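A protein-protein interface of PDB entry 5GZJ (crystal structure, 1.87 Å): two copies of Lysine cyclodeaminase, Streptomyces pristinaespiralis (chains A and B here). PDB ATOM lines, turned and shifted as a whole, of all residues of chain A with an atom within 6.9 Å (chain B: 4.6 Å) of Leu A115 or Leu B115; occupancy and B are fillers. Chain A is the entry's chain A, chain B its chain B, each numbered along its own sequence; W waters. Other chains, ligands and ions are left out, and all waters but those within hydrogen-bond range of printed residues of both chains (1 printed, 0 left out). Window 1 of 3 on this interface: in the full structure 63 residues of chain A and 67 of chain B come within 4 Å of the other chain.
O of Trp A8 sits at hydrogen-bond distance from N of Leu A115 (2.9 Å). N of Leu A10 is in hydrogen-bond range of O of Leu A115. O of Leu A10 is in hydrogen-bond range of N of Asp A117 (3.2 Å). The backbone carbonyl oxygen of Thr A101 sits at hydrogen-bond distance from the backbone NH of Thr A82 (3.0 Å). N of Leu B115 lies within hydrogen-bond range of O of Trp B8 (2.9 Å). The backbone NH (N) of Leu B10 is in hydrogen-bond range of the backbone carbonyl oxygen (O) of Leu B115, 2.9 Å away.
Among the printed residues, pairs that only touch across the chains: Asp A117 with Ile B334 (3.3 Å), Gly A11 with Ile B334 (3.4 Å), Leu A115 with Leu B115 (3.5 Å), Ile A334 with Leu B115 (3.8 Å), Ile A334 with Thr B101 (3.9 Å) and Thr A101 with Ile B334 (3.97 Å).
Printed residues of chain B within 4 Å of Gly A11: Ile B334. Of the printed residues of chain B, Thr A101 touches Ile B334. Leu A115 touches just one residue of chain B: Leu B115 (3.5 Å). Printed residues of chain B within 4 Å of Asp A117: Ile B334. Of the printed residues of chain B, Ile A334 touches Thr B101 and Leu B115. Leu B10 touches none of the printed residues of chain A. Of the printed residues of chain A, Thr B101 touches Ile A334. Of chain A, only Leu A115 and Ile A334 come within 4 Å of Leu B115. Met B116 touches none of the printed residues of chain A. The nearest residue of chain B that does not touch Leu A115 is Ile B334 (4.03 Å).
Of the 12 printed residues of chain B, 3 touch a printed residue of chain A. Of the 21 printed residues of chain A, 5 touch a printed residue of chain B. Hydrophobic or aromatic side chains of chain A within 4 Å of the printed part of chain B: Leu A115 and Ile A334. Along chain A the printed residues that touch a printed residue of chain B span positions 11 to 334.
Thr A101 touches Ile B334, and with the chains exchanged Ile A334 touches Thr B101. Leu A115 touches its own counterpart, Leu B115. Ile A334 touches Leu B115, but with the chains exchanged Leu A115 does not touch Ile B334 (4.03 Å). Positions printed for both chains: 7, 8, 9, 10, 101, 102, 103, 114, 115, 116, 316 and 334. Of the 6 pairs that touch across the chains among the printed residues, 3 have their exchanged pair printed and touching as well.
Water W1 bridges OH of Tyr A105 (2.7 Å) and OG1 of Thr B101 (2.8 Å).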
ATOM      1  N   THR A   7      22.817  -7.827  11.603  1.00  0.00           N
ATOM      2  CA  THR A   7      24.070  -7.457  12.220  1.00  0.00           C
ATOM      3  C   THR A   7      24.960  -8.657  12.444  1.00  0.00           C
ATOM      4  O   THR A   7      24.540  -9.659  13.036  1.00  0.00           O
ATOM      5  CB  THR A   7      23.839  -6.724  13.574  1.00  0.00           C
ATOM      6  OG1 THR A   7      23.002  -5.574  13.367  1.00  0.00           O
ATOM      7  CG2 THR A   7      25.174  -6.260  14.217  1.00  0.00           C
ATOM      8  N   TRP A   8      26.208  -8.547  12.010  1.00  0.00           N
ATOM      9  CA  TRP A   8      27.214  -9.582  12.263  1.00  0.00           C
ATOM     10  C   TRP A   8      27.831  -9.345  13.628  1.00  0.00           C
ATOM     11  O   TRP A   8      28.503  -8.352  13.794  1.00  0.00           O
ATOM     12  CB  TRP A   8      28.268  -9.503  11.156  1.00  0.00           C
ATOM     13  CG  TRP A   8      29.323 -10.534  11.115  1.00  0.00           C
ATOM     14  CD1 TRP A   8      29.267 -11.770  11.650  1.00  0.00           C
ATOM     15  CD2 TRP A   8      30.588 -10.453  10.429  1.00  0.00           C
ATOM     16  NE1 TRP A   8      30.405 -12.466  11.372  1.00  0.00           N
ATOM     17  CE2 TRP A   8      31.239 -11.683  10.621  1.00  0.00           C
ATOM     18  CE3 TRP A   8      31.234  -9.458   9.685  1.00  0.00           C
ATOM     19  CZ2 TRP A   8      32.508 -11.951  10.113  1.00  0.00           C
ATOM     20  CZ3 TRP A   8      32.477  -9.740   9.140  1.00  0.00           C
ATOM     21  CH2 TRP A   8      33.118 -10.972   9.401  1.00  0.00           C
ATOM     22  N   VAL A   9      27.650 -10.288  14.562  1.00  0.00           N
ATOM     23  CA  VAL A   9      28.166 -10.150  15.899  1.00  0.00           C
ATOM     24  C   VAL A   9      29.317 -11.127  16.082  1.00  0.00           C
ATOM     25  O   VAL A   9      29.134 -12.348  15.874  1.00  0.00           O
ATOM     26  CB  VAL A   9      27.060 -10.448  16.929  1.00  0.00           C
ATOM     27  CG1 VAL A   9      27.556 -10.286  18.353  1.00  0.00           C
ATOM     28  CG2 VAL A   9      25.826  -9.550  16.719  1.00  0.00           C
ATOM     29  N   LEU A  10      30.458 -10.580  16.499  1.00  0.00           N
ATOM     30  CA  LEU A  10      31.644 -11.346  16.922  1.00  0.00           C
ATOM     31  C   LEU A  10      31.906 -11.142  18.435  1.00  0.00           C
ATOM     32  O   LEU A  10      32.540 -10.166  18.898  1.00  0.00           O
ATOM     33  CB  LEU A  10      32.875 -10.910  16.175  1.00  0.00           C
ATOM     34  CG  LEU A  10      32.942 -11.058  14.672  1.00  0.00           C
ATOM     35  CD1 LEU A  10      34.274 -10.467  14.219  1.00  0.00           C
ATOM     36  CD2 LEU A  10      32.835 -12.525  14.229  1.00  0.00           C
ATOM     37  N   GLY A  11      31.470 -12.104  19.202  1.00  0.00           N
ATOM     38  CA  GLY A  11      31.697 -12.031  20.636  1.00  0.00           C
ATOM     39  C   GLY A  11      32.916 -12.810  21.076  1.00  0.00           C
ATOM     40  O   GLY A  11      33.785 -13.180  20.297  1.00  0.00           O
ATOM     41  N   LEU A  80      32.028   3.040  16.068  1.00  0.00           N
ATOM     42  CA  LEU A  80      31.830   3.595  17.389  1.00  0.00           C
ATOM     43  C   LEU A  80      32.348   2.629  18.433  1.00  0.00           C
ATOM     44  O   LEU A  80      31.843   1.506  18.518  1.00  0.00           O
ATOM     45  CB  LEU A  80      30.387   3.952  17.699  1.00  0.00           C
ATOM     46  CG  LEU A  80      30.212   4.603  19.095  1.00  0.00           C
ATOM     47  CD1 LEU A  80      30.734   6.014  19.092  1.00  0.00           C
ATOM     48  CD2 LEU A  80      28.749   4.627  19.550  1.00  0.00           C
ATOM     49  N   THR A  82      32.557   2.070  22.432  1.00  0.00           N
ATOM     50  CA  THR A  82      32.013   2.456  23.740  1.00  0.00           C
ATOM     51  C   THR A  82      32.803   1.684  24.806  1.00  0.00           C
ATOM     52  O   THR A  82      32.958   0.458  24.699  1.00  0.00           O
ATOM     53  CB  THR A  82      30.492   2.119  23.842  1.00  0.00           C
ATOM     54  OG1 THR A  82      30.230   0.808  23.373  1.00  0.00           O
ATOM     55  CG2 THR A  82      29.668   3.071  22.985  1.00  0.00           C
ATOM     56  N   THR A 101      33.149  -2.363  23.642  1.00  0.00           N
ATOM     57  CA  THR A 101      32.619  -2.998  22.459  1.00  0.00           C
ATOM     58  C   THR A 101      32.798  -2.007  21.341  1.00  0.00           C
ATOM     59  O   THR A 101      32.870  -0.792  21.568  1.00  0.00           O
ATOM     60  CB  THR A 101      31.103  -3.317  22.558  1.00  0.00           C
ATOM     61  OG1 THR A 101      30.409  -2.202  23.120  1.00  0.00           O
ATOM     62  CG2 THR A 101      30.864  -4.497  23.438  1.00  0.00           C
ATOM     63  N   VAL A 102      32.865  -2.537  20.105  1.00  0.00           N
ATOM     64  CA  VAL A 102      33.075  -1.731  18.891  1.00  0.00           C
ATOM     65  C   VAL A 102      32.013  -2.073  17.888  1.00  0.00           C
ATOM     66  O   VAL A 102      31.705  -3.266  17.636  1.00  0.00           O
ATOM     67  CB  VAL A 102      34.463  -1.962  18.264  1.00  0.00           C
ATOM     68  CG1 VAL A 102      34.812  -0.847  17.292  1.00  0.00           C
ATOM     69  CG2 VAL A 102      35.509  -2.003  19.347  1.00  0.00           C
ATOM     70  N   ALA A 103      31.346  -1.046  17.412  1.00  0.00           N
ATOM     71  CA  ALA A 103      30.258  -1.198  16.431  1.00  0.00           C
ATOM     72  C   ALA A 103      30.611  -0.511  15.116  1.00  0.00           C
ATOM     73  O   ALA A 103      31.358   0.486  15.093  1.00  0.00           O
ATOM     74  CB  ALA A 103      28.944  -0.574  16.953  1.00  0.00           C
ATOM     75  N   ARG A 104      30.048  -1.038  14.047  1.00  0.00           N
ATOM     76  CA  ARG A 104      30.174  -0.450  12.718  1.00  0.00           C
ATOM     77  C   ARG A 104      28.799  -0.228  12.119  1.00  0.00           C
ATOM     78  O   ARG A 104      27.953  -1.129  12.177  1.00  0.00           O
ATOM     79  CB  ARG A 104      31.015  -1.392  11.842  1.00  0.00           C
ATOM     80  CG  ARG A 104      31.219  -0.847  10.427  1.00  0.00           C
ATOM     81  CD  ARG A 104      32.070  -1.788   9.589  1.00  0.00           C
ATOM     82  NE  ARG A 104      33.473  -1.762   9.995  1.00  0.00           N
ATOM     83  CZ  ARG A 104      34.487  -2.313   9.310  1.00  0.00           C
ATOM     84  NH1 ARG A 104      34.273  -3.048   8.241  1.00  0.00           N
ATOM     85  NH2 ARG A 104      35.712  -2.227   9.797  1.00  0.00           N
ATOM     86  N   TYR A 105      28.588   0.968  11.550  1.00  0.00           N
ATOM     87  CA  TYR A 105      27.348   1.365  10.941  1.00  0.00           C
ATOM     88  C   TYR A 105      27.644   1.761   9.491  1.00  0.00           C
ATOM     89  O   TYR A 105      28.674   2.426   9.189  1.00  0.00           O
ATOM     90  CB  TYR A 105      26.773   2.568  11.659  1.00  0.00           C
ATOM     91  CG  TYR A 105      26.631   2.356  13.152  1.00  0.00           C
ATOM     92  CD1 TYR A 105      27.728   2.495  14.005  1.00  0.00           C
ATOM     93  CD2 TYR A 105      25.398   2.034  13.718  1.00  0.00           C
ATOM     94  CE1 TYR A 105      27.604   2.253  15.367  1.00  0.00           C
ATOM     95  CE2 TYR A 105      25.269   1.787  15.082  1.00  0.00           C
ATOM     96  CZ  TYR A 105      26.375   1.935  15.907  1.00  0.00           C
ATOM     97  OH  TYR A 105      26.232   1.671  17.257  1.00  0.00           O
ATOM     98  N   LEU A 112      23.327  -0.633  11.537  1.00  0.00           N
ATOM     99  CA  LEU A 112      24.352  -1.368  12.335  1.00  0.00           C
ATOM    100  C   LEU A 112      24.753  -2.699  11.615  1.00  0.00           C
ATOM    101  O   LEU A 112      23.916  -3.624  11.494  1.00  0.00           O
ATOM    102  CB  LEU A 112      23.814  -1.697  13.704  1.00  0.00           C
ATOM    103  CG  LEU A 112      24.686  -2.596  14.646  1.00  0.00           C
ATOM    104  CD1 LEU A 112      25.947  -1.862  15.029  1.00  0.00           C
ATOM    105  CD2 LEU A 112      23.912  -3.031  15.894  1.00  0.00           C
ATOM    106  N   THR A 113      25.976  -2.793  11.125  1.00  0.00           N
ATOM    107  CA  THR A 113      26.334  -3.940  10.314  1.00  0.00           C
ATOM    108  C   THR A 113      27.178  -4.938  11.046  1.00  0.00           C
ATOM    109  O   THR A 113      27.246  -6.075  10.644  1.00  0.00           O
ATOM    110  CB  THR A 113      27.054  -3.525   9.004  1.00  0.00           C
ATOM    111  OG1 THR A 113      28.246  -2.799   9.319  1.00  0.00           O
ATOM    112  CG2 THR A 113      26.116  -2.659   8.221  1.00  0.00           C
ATOM    113  N   ALA A 114      27.899  -4.510  12.067  1.00  0.00           N
ATOM    114  CA  ALA A 114      28.782  -5.391  12.817  1.00  0.00           C
ATOM    115  C   ALA A 114      29.016  -4.901  14.239  1.00  0.00           C
ATOM    116  O   ALA A 114      29.007  -3.706  14.487  1.00  0.00           O
ATOM    117  CB  ALA A 114      30.104  -5.551  12.118  1.00  0.00           C
ATOM    118  N   LEU A 115      29.221  -5.841  15.160  1.00  0.00           N
ATOM    119  CA  LEU A 115      29.417  -5.498  16.581  1.00  0.00           C
ATOM    120  C   LEU A 115      30.330  -6.583  17.201  1.00  0.00           C
ATOM    121  O   LEU A 115      30.161  -7.780  16.901  1.00  0.00           O
ATOM    122  CB  LEU A 115      28.069  -5.526  17.281  1.00  0.00           C
ATOM    123  CG  LEU A 115      28.016  -5.289  18.794  1.00  0.00           C
ATOM    124  CD1 LEU A 115      28.432  -3.898  19.209  1.00  0.00           C
ATOM    125  CD2 LEU A 115      26.591  -5.548  19.290  1.00  0.00           C
ATOM    126  N   MET A 116      31.350  -6.155  17.960  1.00  0.00           N
ATOM    127  CA  MET A 116      32.299  -7.125  18.503  1.00  0.00           C
ATOM    128  C   MET A 116      32.885  -6.648  19.784  1.00  0.00           C
ATOM    129  O   MET A 116      32.783  -5.422  20.161  1.00  0.00           O
ATOM    130  CB  MET A 116      33.466  -7.397  17.512  1.00  0.00           C
ATOM    131  CG  MET A 116      34.339  -6.219  17.219  1.00  0.00           C
ATOM    132  SD  MET A 116      35.818  -6.616  16.247  1.00  0.00           S
ATOM    133  CE  MET A 116      36.754  -7.667  17.416  1.00  0.00           C
ATOM    134  N   ASP A 117      33.515  -7.600  20.485  1.00  0.00           N
ATOM    135  CA  ASP A 117      34.301  -7.287  21.655  1.00  0.00           C
ATOM    136  C   ASP A 117      35.272  -6.156  21.426  1.00  0.00           C
ATOM    137  O   ASP A 117      35.910  -6.104  20.385  1.00  0.00           O
ATOM    138  CB  ASP A 117      35.094  -8.483  22.108  1.00  0.00           C
ATOM    139  CG  ASP A 117      36.031  -8.140  23.219  1.00  0.00           C
ATOM    140  OD1 ASP A 117      35.537  -7.575  24.251  1.00  0.00           O
ATOM    141  OD2 ASP A 117      37.274  -8.407  23.079  1.00  0.00           O
ATOM    142  N   MET A 316      39.536  -3.431  14.261  1.00  0.00           N
ATOM    143  CA  MET A 316      38.326  -4.174  13.930  1.00  0.00           C
ATOM    144  C   MET A 316      38.357  -4.814  12.518  1.00  0.00           C
ATOM    145  O   MET A 316      37.900  -5.976  12.346  1.00  0.00           O
ATOM    146  CB  MET A 316      37.077  -3.279  14.079  1.00  0.00           C
ATOM    147  CG  MET A 316      35.768  -3.934  13.718  1.00  0.00           C
ATOM    148  SD  MET A 316      34.371  -3.032  14.488  1.00  0.00           S
ATOM    149  CE  MET A 316      32.939  -4.008  14.071  1.00  0.00           C
ATOM    150  N   LEU A 320      37.660  -8.596  11.476  1.00  0.00           N
ATOM    151  CA  LEU A 320      36.593  -8.920  10.509  1.00  0.00           C
ATOM    152  C   LEU A 320      37.127  -9.714   9.313  1.00  0.00           C
ATOM    153  O   LEU A 320      36.491 -10.684   8.896  1.00  0.00           O
ATOM    154  CB  LEU A 320      35.836  -7.662  10.044  1.00  0.00           C
ATOM    155  CG  LEU A 320      35.035  -6.906  11.150  1.00  0.00           C
ATOM    156  CD1 LEU A 320      34.290  -5.760  10.475  1.00  0.00           C
ATOM    157  CD2 LEU A 320      34.078  -7.799  11.861  1.00  0.00           C
ATOM    158  N   ILE A 334      18.822  -7.158  14.696  1.00  0.00           N
ATOM    159  CA  ILE A 334      18.624  -6.345  15.908  1.00  0.00           C
ATOM    160  C   ILE A 334      17.706  -5.184  15.593  1.00  0.00           C
ATOM    161  O   ILE A 334      16.670  -5.009  16.251  1.00  0.00           O
ATOM    162  CB  ILE A 334      19.965  -5.825  16.484  1.00  0.00           C
ATOM    163  CG1 ILE A 334      20.853  -7.000  16.866  1.00  0.00           C
ATOM    164  CG2 ILE A 334      19.701  -4.934  17.732  1.00  0.00           C
ATOM    165  CD1 ILE A 334      22.243  -6.592  17.313  1.00  0.00           C
ATOM    166  N   THR B   7      25.278 -10.087  27.390  1.00  0.00           N
ATOM    167  CA  THR B   7      24.424  -9.010  26.960  1.00  0.00           C
ATOM    168  C   THR B   7      23.070  -9.652  26.531  1.00  0.00           C
ATOM    169  O   THR B   7      23.026 -10.606  25.765  1.00  0.00           O
ATOM    170  CB  THR B   7      25.016  -8.312  25.734  1.00  0.00           C
ATOM    171  OG1 THR B   7      26.313  -7.798  26.062  1.00  0.00           O
ATOM    172  CG2 THR B   7      24.088  -7.211  25.282  1.00  0.00           C
ATOM    173  N   TRP B   8      22.017  -9.044  27.003  1.00  0.00           N
ATOM    174  CA  TRP B   8      20.651  -9.400  26.654  1.00  0.00           C
ATOM    175  C   TRP B   8      20.299  -8.623  25.387  1.00  0.00           C
ATOM    176  O   TRP B   8      20.202  -7.397  25.405  1.00  0.00           O
ATOM    177  CB  TRP B   8      19.766  -8.977  27.824  1.00  0.00           C
ATOM    178  CG  TRP B   8      18.307  -9.384  27.707  1.00  0.00           C
ATOM    179  CD1 TRP B   8      17.800 -10.352  26.935  1.00  0.00           C
ATOM    180  CD2 TRP B   8      17.219  -8.831  28.426  1.00  0.00           C
ATOM    181  NE1 TRP B   8      16.431 -10.430  27.106  1.00  0.00           N
ATOM    182  CE2 TRP B   8      16.065  -9.517  28.039  1.00  0.00           C
ATOM    183  CE3 TRP B   8      17.115  -7.843  29.386  1.00  0.00           C
ATOM    184  CZ2 TRP B   8      14.811  -9.237  28.576  1.00  0.00           C
ATOM    185  CZ3 TRP B   8      15.859  -7.533  29.889  1.00  0.00           C
ATOM    186  CH2 TRP B   8      14.744  -8.210  29.479  1.00  0.00           C
ATOM    187  N   VAL B   9      20.098  -9.349  24.309  1.00  0.00           N
ATOM    188  CA  VAL B   9      19.754  -8.772  23.024  1.00  0.00           C
ATOM    189  C   VAL B   9      18.285  -9.023  22.692  1.00  0.00           C
ATOM    190  O   VAL B   9      17.840 -10.165  22.620  1.00  0.00           O
ATOM    191  CB  VAL B   9      20.650  -9.296  21.896  1.00  0.00           C
ATOM    192  CG1 VAL B   9      20.285  -8.539  20.623  1.00  0.00           C
ATOM    193  CG2 VAL B   9      22.122  -9.035  22.267  1.00  0.00           C
ATOM    194  N   LEU B  10      17.568  -7.926  22.578  1.00  0.00           N
ATOM    195  CA  LEU B  10      16.185  -7.869  22.044  1.00  0.00           C
ATOM    196  C   LEU B  10      16.221  -7.319  20.637  1.00  0.00           C
ATOM    197  O   LEU B  10      16.291  -6.078  20.428  1.00  0.00           O
ATOM    198  CB  LEU B  10      15.302  -6.950  22.878  1.00  0.00           C
ATOM    199  CG  LEU B  10      15.056  -7.414  24.329  1.00  0.00           C
ATOM    200  CD1 LEU B  10      14.282  -6.344  25.082  1.00  0.00           C
ATOM    201  CD2 LEU B  10      14.249  -8.726  24.354  1.00  0.00           C
ATOM    202  N   THR B 101      19.545   1.944  17.338  1.00  0.00           N
ATOM    203  CA  THR B 101      19.596   0.869  18.357  1.00  0.00           C
ATOM    204  C   THR B 101      19.811   1.545  19.685  1.00  0.00           C
ATOM    205  O   THR B 101      20.352   2.681  19.735  1.00  0.00           O
ATOM    206  CB  THR B 101      20.742  -0.143  18.082  1.00  0.00           C
ATOM    207  OG1 THR B 101      21.883   0.513  17.571  1.00  0.00           O
ATOM    208  CG2 THR B 101      20.370  -1.140  16.979  1.00  0.00           C
ATOM    209  N   VAL B 102      19.398   0.882  20.782  1.00  0.00           N
ATOM    210  CA  VAL B 102      19.557   1.434  22.116  1.00  0.00           C
ATOM    211  C   VAL B 102      20.279   0.404  22.979  1.00  0.00           C
ATOM    212  O   VAL B 102      19.892  -0.772  22.996  1.00  0.00           O
ATOM    213  CB  VAL B 102      18.214   1.797  22.748  1.00  0.00           C
ATOM    214  CG1 VAL B 102      18.417   2.742  23.915  1.00  0.00           C
ATOM    215  CG2 VAL B 102      17.338   2.505  21.745  1.00  0.00           C
ATOM    216  N   ALA B 103      21.309   0.840  23.657  1.00  0.00           N
ATOM    217  CA  ALA B 103      22.132  -0.038  24.495  1.00  0.00           C
ATOM    218  C   ALA B 103      22.098   0.447  25.945  1.00  0.00           C
ATOM    219  O   ALA B 103      21.928   1.627  26.198  1.00  0.00           O
ATOM    220  CB  ALA B 103      23.553   0.002  23.958  1.00  0.00           C
ATOM    221  N   ALA B 114      22.502  -4.771  27.918  1.00  0.00           N
ATOM    222  CA  ALA B 114      21.330  -4.928  27.042  1.00  0.00           C
ATOM    223  C   ALA B 114      21.478  -4.141  25.745  1.00  0.00           C
ATOM    224  O   ALA B 114      22.105  -3.081  25.737  1.00  0.00           O
ATOM    225  CB  ALA B 114      20.057  -4.551  27.776  1.00  0.00           C
ATOM    226  N   LEU B 115      20.887  -4.657  24.663  1.00  0.00           N
ATOM    227  CA  LEU B 115      20.912  -3.986  23.363  1.00  0.00           C
ATOM    228  C   LEU B 115      19.628  -4.324  22.651  1.00  0.00           C
ATOM    229  O   LEU B 115      19.203  -5.478  22.640  1.00  0.00           O
ATOM    230  CB  LEU B 115      22.091  -4.508  22.549  1.00  0.00           C
ATOM    231  CG  LEU B 115      22.269  -3.998  21.124  1.00  0.00           C
ATOM    232  CD1 LEU B 115      22.478  -2.490  21.069  1.00  0.00           C
ATOM    233  CD2 LEU B 115      23.434  -4.717  20.457  1.00  0.00           C
ATOM    234  N   MET B 116      18.983  -3.329  22.062  1.00  0.00           N
ATOM    235  CA  MET B 116      17.751  -3.566  21.382  1.00  0.00           C
ATOM    236  C   MET B 116      17.544  -2.613  20.222  1.00  0.00           C
ATOM    237  O   MET B 116      18.223  -1.585  20.070  1.00  0.00           O
ATOM    238  CB  MET B 116      16.563  -3.424  22.378  1.00  0.00           C
ATOM    239  CG  MET B 116      16.370  -2.019  22.952  1.00  0.00           C
ATOM    240  SD  MET B 116      14.798  -1.807  23.904  1.00  0.00           S
ATOM    241  CE  MET B 116      13.669  -2.141  22.579  1.00  0.00           C
ATOM    242  N   MET B 316      12.894   2.313  26.752  1.00  0.00           N
ATOM    243  CA  MET B 316      13.588   1.037  26.788  1.00  0.00           C
ATOM    244  C   MET B 316      13.163   0.238  28.029  1.00  0.00           C
ATOM    245  O   MET B 316      12.946  -0.967  27.925  1.00  0.00           O
ATOM    246  CB  MET B 316      15.108   1.237  26.706  1.00  0.00           C
ATOM    247  CG  MET B 316      15.856  -0.079  26.802  1.00  0.00           C
ATOM    248  SD  MET B 316      17.579   0.140  26.325  1.00  0.00           S
ATOM    249  CE  MET B 316      18.258  -1.524  26.447  1.00  0.00           C
ATOM    250  N   ILE B 334      29.317 -10.976  24.339  1.00  0.00           N
ATOM    251  CA  ILE B 334      29.959 -10.153  23.354  1.00  0.00           C
ATOM    252  C   ILE B 334      31.313  -9.674  23.885  1.00  0.00           C
ATOM    253  O   ILE B 334      32.330  -9.864  23.204  1.00  0.00           O
ATOM    254  CB  ILE B 334      29.069  -8.940  22.986  1.00  0.00           C
ATOM    255  CG1 ILE B 334      27.759  -9.463  22.387  1.00  0.00           C
ATOM    256  CG2 ILE B 334      29.714  -7.991  21.953  1.00  0.00           C
ATOM    257  CD1 ILE B 334      26.749  -8.341  22.188  1.00  0.00           C
HETATM  258  O   HOH W   1      24.491  -0.218  18.212  1.00  0.00           O
